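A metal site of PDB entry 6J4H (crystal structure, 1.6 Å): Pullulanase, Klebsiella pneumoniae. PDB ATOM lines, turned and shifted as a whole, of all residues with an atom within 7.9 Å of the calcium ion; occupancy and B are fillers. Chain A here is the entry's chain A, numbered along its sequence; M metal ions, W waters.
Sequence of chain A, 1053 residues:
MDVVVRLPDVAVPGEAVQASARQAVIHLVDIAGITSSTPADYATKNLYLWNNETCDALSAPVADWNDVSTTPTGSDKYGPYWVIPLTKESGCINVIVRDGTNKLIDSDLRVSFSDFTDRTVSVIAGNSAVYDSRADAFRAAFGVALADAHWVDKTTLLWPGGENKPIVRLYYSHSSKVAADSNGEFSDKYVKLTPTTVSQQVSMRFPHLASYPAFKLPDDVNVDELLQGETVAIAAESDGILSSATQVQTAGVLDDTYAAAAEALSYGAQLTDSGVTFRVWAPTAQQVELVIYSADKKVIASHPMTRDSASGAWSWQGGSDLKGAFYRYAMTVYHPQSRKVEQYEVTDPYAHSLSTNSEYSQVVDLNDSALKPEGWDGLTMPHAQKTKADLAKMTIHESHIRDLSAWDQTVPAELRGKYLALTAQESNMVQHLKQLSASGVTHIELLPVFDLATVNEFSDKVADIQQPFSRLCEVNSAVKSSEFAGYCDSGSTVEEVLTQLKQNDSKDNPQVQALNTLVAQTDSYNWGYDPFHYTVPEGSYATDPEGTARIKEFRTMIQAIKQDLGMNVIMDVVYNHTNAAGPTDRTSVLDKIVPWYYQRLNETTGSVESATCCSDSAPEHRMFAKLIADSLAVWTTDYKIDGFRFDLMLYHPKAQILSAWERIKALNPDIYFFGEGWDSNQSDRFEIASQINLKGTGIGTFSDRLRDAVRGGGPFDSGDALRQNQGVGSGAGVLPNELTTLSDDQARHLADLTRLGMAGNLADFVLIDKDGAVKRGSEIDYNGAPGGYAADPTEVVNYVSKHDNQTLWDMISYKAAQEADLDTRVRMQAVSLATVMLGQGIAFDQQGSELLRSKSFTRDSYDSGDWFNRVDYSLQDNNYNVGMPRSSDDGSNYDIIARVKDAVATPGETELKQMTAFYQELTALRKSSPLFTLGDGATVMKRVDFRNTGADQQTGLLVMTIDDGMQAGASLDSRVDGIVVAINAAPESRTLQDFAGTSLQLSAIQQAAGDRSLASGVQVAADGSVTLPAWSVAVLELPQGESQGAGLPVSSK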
ATOM      1  N   THR A 454     -11.798   1.158 -18.500  1.00  0.00           N
ATOM      2  CA  THR A 454     -12.215  -0.009 -17.734  1.00  0.00           C
ATOM      3  C   THR A 454     -12.973   0.334 -16.452  1.00  0.00           C
ATOM      4  O   THR A 454     -13.142  -0.518 -15.575  1.00  0.00           O
ATOM      5  CB  THR A 454     -10.996  -0.864 -17.421  1.00  0.00           C
ATOM      6  OG1 THR A 454      -9.902  -0.010 -17.051  1.00  0.00           O
ATOM      7  CG2 THR A 454     -10.602  -1.669 -18.658  1.00  0.00           C
ATOM      8  N   VAL A 455     -13.433   1.581 -16.323  1.00  0.00           N
ATOM      9  CA  VAL A 455     -14.443   1.965 -15.348  1.00  0.00           C
ATOM     10  C   VAL A 455     -15.612   2.595 -16.113  1.00  0.00           C
ATOM     11  O   VAL A 455     -15.389   3.429 -17.003  1.00  0.00           O
ATOM     12  CB  VAL A 455     -13.903   2.937 -14.281  1.00  0.00           C
ATOM     13  CG1 VAL A 455     -15.007   3.381 -13.344  1.00  0.00           C
ATOM     14  CG2 VAL A 455     -12.776   2.269 -13.474  1.00  0.00           C
ATOM     15  N   ASN A 456     -16.834   2.174 -15.803  1.00  0.00           N
ATOM     16  CA  ASN A 456     -17.992   2.780 -16.430  1.00  0.00           C
ATOM     17  C   ASN A 456     -18.246   4.117 -15.755  1.00  0.00           C
ATOM     18  O   ASN A 456     -18.399   4.188 -14.530  1.00  0.00           O
ATOM     19  CB  ASN A 456     -19.212   1.864 -16.314  1.00  0.00           C
ATOM     20  CG  ASN A 456     -20.342   2.285 -17.213  1.00  0.00           C
ATOM     21  OD1 ASN A 456     -20.620   3.475 -17.357  1.00  0.00           O
ATOM     22  ND2 ASN A 456     -21.017   1.320 -17.824  1.00  0.00           N
ATOM     23  N   ASP A 464     -20.123   0.115  -5.721  1.00  0.00           N
ATOM     24  CA  ASP A 464     -18.888   0.030  -4.949  1.00  0.00           C
ATOM     25  C   ASP A 464     -19.166  -0.623  -3.601  1.00  0.00           C
ATOM     26  O   ASP A 464     -20.322  -0.789  -3.196  1.00  0.00           O
ATOM     27  CB  ASP A 464     -18.259   1.404  -4.794  1.00  0.00           C
ATOM     28  CG  ASP A 464     -17.570   1.834  -6.077  1.00  0.00           C
ATOM     29  OD1 ASP A 464     -16.607   1.133  -6.471  1.00  0.00           O
ATOM     30  OD2 ASP A 464     -18.000   2.835  -6.688  1.00  0.00           O
ATOM     31  N   ASN A 516     -15.157 -10.878  -4.465  1.00  0.00           N
ATOM     32  CA  ASN A 516     -14.543  -9.658  -4.945  1.00  0.00           C
ATOM     33  C   ASN A 516     -14.248  -9.698  -6.435  1.00  0.00           C
ATOM     34  O   ASN A 516     -14.269  -8.660  -7.097  1.00  0.00           O
ATOM     35  CB  ASN A 516     -13.256  -9.374  -4.170  1.00  0.00           C
ATOM     36  CG  ASN A 516     -12.855  -7.929  -4.273  1.00  0.00           C
ATOM     37  OD1 ASN A 516     -13.634  -7.043  -3.899  1.00  0.00           O
ATOM     38  ND2 ASN A 516     -11.637  -7.659  -4.755  1.00  0.00           N
ATOM     39  N   THR A 517     -13.962 -10.887  -6.979  1.00  0.00           N
ATOM     40  CA  THR A 517     -13.742 -11.005  -8.415  1.00  0.00           C
ATOM     41  C   THR A 517     -14.987 -10.604  -9.211  1.00  0.00           C
ATOM     42  O   THR A 517     -14.872 -10.058 -10.315  1.00  0.00           O
ATOM     43  CB  THR A 517     -13.318 -12.437  -8.761  1.00  0.00           C
ATOM     44  OG1 THR A 517     -12.043 -12.710  -8.152  1.00  0.00           O
ATOM     45  CG2 THR A 517     -13.208 -12.633 -10.273  1.00  0.00           C
ATOM     46  N   LEU A 518     -16.175 -10.869  -8.660  1.00  0.00           N
ATOM     47  CA  LEU A 518     -17.398 -10.435  -9.307  1.00  0.00           C
ATOM     48  C   LEU A 518     -17.608  -8.927  -9.148  1.00  0.00           C
ATOM     49  O   LEU A 518     -17.953  -8.228 -10.114  1.00  0.00           O
ATOM     50  CB  LEU A 518     -18.584 -11.220  -8.725  1.00  0.00           C
ATOM     51  CG  LEU A 518     -18.400 -12.733  -8.830  1.00  0.00           C
ATOM     52  CD1 LEU A 518     -19.619 -13.463  -8.265  1.00  0.00           C
ATOM     53  CD2 LEU A 518     -18.160 -13.156 -10.271  1.00  0.00           C
ATOM     54  N   VAL A 519     -17.412  -8.420  -7.921  1.00  0.00           N
ATOM     55  CA  VAL A 519     -17.491  -6.991  -7.641  1.00  0.00           C
ATOM     56  C   VAL A 519     -16.635  -6.193  -8.614  1.00  0.00           C
ATOM     57  O   VAL A 519     -17.032  -5.119  -9.076  1.00  0.00           O
ATOM     58  CB  VAL A 519     -17.048  -6.724  -6.192  1.00  0.00           C
ATOM     59  CG1 VAL A 519     -16.839  -5.226  -5.934  1.00  0.00           C
ATOM     60  CG2 VAL A 519     -18.046  -7.318  -5.191  1.00  0.00           C
ATOM     61  N   ALA A 520     -15.454  -6.711  -8.930  1.00  0.00           N
ATOM     62  CA  ALA A 520     -14.488  -6.000  -9.757  1.00  0.00           C
ATOM     63  C   ALA A 520     -15.032  -5.674 -11.152  1.00  0.00           C
ATOM     64  O   ALA A 520     -14.533  -4.732 -11.794  1.00  0.00           O
ATOM     65  CB  ALA A 520     -13.212  -6.828  -9.879  1.00  0.00           C
ATOM     66  N   GLN A 521     -16.022  -6.422 -11.624  1.00  0.00           N
ATOM     67  CA  GLN A 521     -16.566  -6.222 -12.967  1.00  0.00           C
ATOM     68  C   GLN A 521     -17.344  -4.921 -13.097  1.00  0.00           C
ATOM     69  O   GLN A 521     -17.481  -4.381 -14.203  1.00  0.00           O
ATOM     70  CB  GLN A 521     -17.476  -7.404 -13.354  1.00  0.00           C
ATOM     71  CG  GLN A 521     -16.820  -8.764 -13.311  1.00  0.00           C
ATOM     72  CD  GLN A 521     -17.829  -9.902 -13.423  1.00  0.00           C
ATOM     73  OE1 GLN A 521     -19.031  -9.671 -13.353  1.00  0.00           O
ATOM     74  NE2 GLN A 521     -17.339 -11.129 -13.588  1.00  0.00           N
ATOM     75  N   THR A 522     -17.896  -4.424 -11.991  1.00  0.00           N
ATOM     76  CA  THR A 522     -18.815  -3.299 -12.052  1.00  0.00           C
ATOM     77  C   THR A 522     -18.523  -2.245 -10.987  1.00  0.00           C
ATOM     78  O   THR A 522     -19.393  -1.420 -10.690  1.00  0.00           O
ATOM     79  CB  THR A 522     -20.287  -3.767 -11.911  1.00  0.00           C
ATOM     80  OG1 THR A 522     -20.402  -4.618 -10.765  1.00  0.00           O
ATOM     81  CG2 THR A 522     -20.745  -4.538 -13.132  1.00  0.00           C
ATOM     82  N   ASP A 523     -17.300  -2.212 -10.417  1.00  0.00           N
ATOM     83  CA  ASP A 523     -16.969  -1.216  -9.417  1.00  0.00           C
ATOM     84  C   ASP A 523     -16.270  -0.028 -10.073  1.00  0.00           C
ATOM     85  O   ASP A 523     -16.142   0.059 -11.298  1.00  0.00           O
ATOM     86  CB  ASP A 523     -16.139  -1.819  -8.275  1.00  0.00           C
ATOM     87  CG  ASP A 523     -14.755  -2.323  -8.697  1.00  0.00           C
ATOM     88  OD1 ASP A 523     -14.295  -2.046  -9.826  1.00  0.00           O
ATOM     89  OD2 ASP A 523     -14.107  -3.012  -7.877  1.00  0.00           O
ATOM     90  N   SER A 524     -15.835   0.915  -9.251  1.00  0.00           N
ATOM     91  CA  SER A 524     -15.127   2.105  -9.717  1.00  0.00           C
ATOM     92  C   SER A 524     -13.621   1.900  -9.833  1.00  0.00           C
ATOM     93  O   SER A 524     -12.910   2.869 -10.096  1.00  0.00           O
ATOM     94  CB  SER A 524     -15.404   3.290  -8.786  1.00  0.00           C
ATOM     95  OG  SER A 524     -16.774   3.649  -8.779  1.00  0.00           O
ATOM     96  N   TYR A 525     -13.117   0.675  -9.635  1.00  0.00           N
ATOM     97  CA  TYR A 525     -11.696   0.467  -9.390  1.00  0.00           C
ATOM     98  C   TYR A 525     -10.994  -0.118 -10.611  1.00  0.00           C
ATOM     99  O   TYR A 525     -11.343  -1.195 -11.090  1.00  0.00           O
ATOM    100  CB  TYR A 525     -11.444  -0.465  -8.177  1.00  0.00           C
ATOM    101  CG  TYR A 525      -9.989  -0.362  -7.784  1.00  0.00           C
ATOM    102  CD1 TYR A 525      -8.995  -1.063  -8.480  1.00  0.00           C
ATOM    103  CD2 TYR A 525      -9.595   0.501  -6.775  1.00  0.00           C
ATOM    104  CE1 TYR A 525      -7.660  -0.922  -8.169  1.00  0.00           C
ATOM    105  CE2 TYR A 525      -8.245   0.645  -6.447  1.00  0.00           C
ATOM    106  CZ  TYR A 525      -7.291  -0.073  -7.147  1.00  0.00           C
ATOM    107  OH  TYR A 525      -5.951   0.074  -6.877  1.00  0.00           O
ATOM    108  N   ASN A 526      -9.933   0.562 -11.061  1.00  0.00           N
ATOM    109  CA  ASN A 526      -8.944  -0.044 -11.941  1.00  0.00           C
ATOM    110  C   ASN A 526      -7.702   0.830 -11.907  1.00  0.00           C
ATOM    111  O   ASN A 526      -7.823   2.047 -11.791  1.00  0.00           O
ATOM    112  CB  ASN A 526      -9.453  -0.170 -13.394  1.00  0.00           C
ATOM    113  CG  ASN A 526      -8.686  -1.223 -14.194  1.00  0.00           C
ATOM    114  OD1 ASN A 526      -7.543  -0.994 -14.604  1.00  0.00           O
ATOM    115  ND2 ASN A 526      -9.315  -2.368 -14.425  1.00  0.00           N
ATOM    116  N   TRP A 527      -6.526   0.205 -12.009  1.00  0.00           N
ATOM    117  CA  TRP A 527      -5.310   0.987 -12.216  1.00  0.00           C
ATOM    118  C   TRP A 527      -5.465   1.903 -13.415  1.00  0.00           C
ATOM    119  O   TRP A 527      -4.982   3.047 -13.410  1.00  0.00           O
ATOM    120  CB  TRP A 527      -4.104   0.090 -12.434  1.00  0.00           C
ATOM    121  CG  TRP A 527      -3.584  -0.565 -11.209  1.00  0.00           C
ATOM    122  CD1 TRP A 527      -3.912  -0.302  -9.915  1.00  0.00           C
ATOM    123  CD2 TRP A 527      -2.604  -1.607 -11.180  1.00  0.00           C
ATOM    124  NE1 TRP A 527      -3.193  -1.118  -9.073  1.00  0.00           N
ATOM    125  CE2 TRP A 527      -2.392  -1.944  -9.835  1.00  0.00           C
ATOM    126  CE3 TRP A 527      -1.900  -2.293 -12.176  1.00  0.00           C
ATOM    127  CZ2 TRP A 527      -1.509  -2.940  -9.445  1.00  0.00           C
ATOM    128  CZ3 TRP A 527      -1.031  -3.293 -11.802  1.00  0.00           C
ATOM    129  CH2 TRP A 527      -0.844  -3.614 -10.451  1.00  0.00           C
ATOM    130  N   TYR A 862      -4.427  -4.914 -10.154  1.00  0.00           N
ATOM    131  CA  TYR A 862      -4.998  -3.879 -11.019  1.00  0.00           C
ATOM    132  C   TYR A 862      -6.519  -3.828 -10.988  1.00  0.00           C
ATOM    133  O   TYR A 862      -7.105  -2.769 -11.217  1.00  0.00           O
ATOM    134  CB  TYR A 862      -4.548  -4.095 -12.469  1.00  0.00           C
ATOM    135  CG  TYR A 862      -5.198  -5.263 -13.155  1.00  0.00           C
ATOM    136  CD1 TYR A 862      -4.775  -6.573 -12.895  1.00  0.00           C
ATOM    137  CD2 TYR A 862      -6.202  -5.070 -14.087  1.00  0.00           C
ATOM    138  CE1 TYR A 862      -5.364  -7.641 -13.532  1.00  0.00           C
ATOM    139  CE2 TYR A 862      -6.797  -6.143 -14.718  1.00  0.00           C
ATOM    140  CZ  TYR A 862      -6.373  -7.423 -14.447  1.00  0.00           C
ATOM    141  OH  TYR A 862      -6.958  -8.478 -15.084  1.00  0.00           O
ATOM    142  N   ASP A 863      -7.165  -4.974 -10.756  1.00  0.00           N
ATOM    143  CA  ASP A 863      -8.617  -5.050 -10.756  1.00  0.00           C
ATOM    144  C   ASP A 863      -9.103  -5.687  -9.463  1.00  0.00           C
ATOM    145  O   ASP A 863     -10.208  -6.241  -9.423  1.00  0.00           O
ATOM    146  CB  ASP A 863      -9.116  -5.837 -11.981  1.00  0.00           C
ATOM    147  CG  ASP A 863     -10.564  -5.527 -12.375  1.00  0.00           C
ATOM    148  OD1 ASP A 863     -11.150  -4.538 -11.905  1.00  0.00           O
ATOM    149  OD2 ASP A 863     -11.122  -6.295 -13.194  1.00  0.00           O
ATOM    150  N   SER A 864      -8.298  -5.635  -8.403  1.00  0.00           N
ATOM    151  CA  SER A 864      -8.635  -6.263  -7.139  1.00  0.00           C
ATOM    152  C   SER A 864      -9.388  -5.324  -6.194  1.00  0.00           C
ATOM    153  O   SER A 864      -9.606  -5.679  -5.034  1.00  0.00           O
ATOM    154  CB  SER A 864      -7.372  -6.814  -6.476  1.00  0.00           C
ATOM    155  OG  SER A 864      -6.923  -7.976  -7.154  1.00  0.00           O
ATOM    156  N   GLY A 865      -9.791  -4.151  -6.674  1.00  0.00           N
ATOM    157  CA  GLY A 865     -10.772  -3.342  -5.985  1.00  0.00           C
ATOM    158  C   GLY A 865     -10.264  -2.573  -4.783  1.00  0.00           C
ATOM    159  O   GLY A 865      -9.091  -2.608  -4.408  1.00  0.00           O
ATOM    160  N   ASP A 866     -11.195  -1.841  -4.166  1.00  0.00           N
ATOM    161  CA  ASP A 866     -10.903  -1.164  -2.909  1.00  0.00           C
ATOM    162  C   ASP A 866     -10.444  -2.144  -1.837  1.00  0.00           C
ATOM    163  O   ASP A 866      -9.654  -1.778  -0.957  1.00  0.00           O
ATOM    164  CB  ASP A 866     -12.137  -0.424  -2.395  1.00  0.00           C
ATOM    165  CG  ASP A 866     -12.547   0.737  -3.273  1.00  0.00           C
ATOM    166  OD1 ASP A 866     -11.711   1.254  -4.053  1.00  0.00           O
ATOM    167  OD2 ASP A 866     -13.714   1.150  -3.153  1.00  0.00           O
HETATM  168 CA    CA M   1     -12.832  -2.970 -11.527  1.00  0.00          CA
HETATM  169  O   HOH W   1     -11.936  -3.784  -9.352  1.00  0.00           O
HETATM  170  O   HOH W   2     -14.344  -1.468 -12.686  1.00  0.00           O
HETATM  171  O   HOH W   3     -12.222  -2.740 -13.863  1.00  0.00           O
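The nearest printed residue that does not touch the calcium ion is Asn 526 (4.6 Å).
Water W1 lies within hydrogen-bond range of OD2 of Asp 523 (2.7 Å), O of Asp 863 (3.0 Å) and N of Gly 865 (3.5 Å). Water W3 lies within hydrogen-bond range of O of Thr 454 (3.0 Å) and ND2 of Asn 526 (3.0 Å). Water W2 lies within hydrogen-bond range of O of Asp 523 (2.7 Å) and O of Thr 454 (3.3 Å).
The calcium ion is bound by OD1 of Asp 863, O of Tyr 525, water W3, water W2, OD1 of Asp 523, O of Ala 520 and water W1. The calcium ion has seven donor atoms within binding distance.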
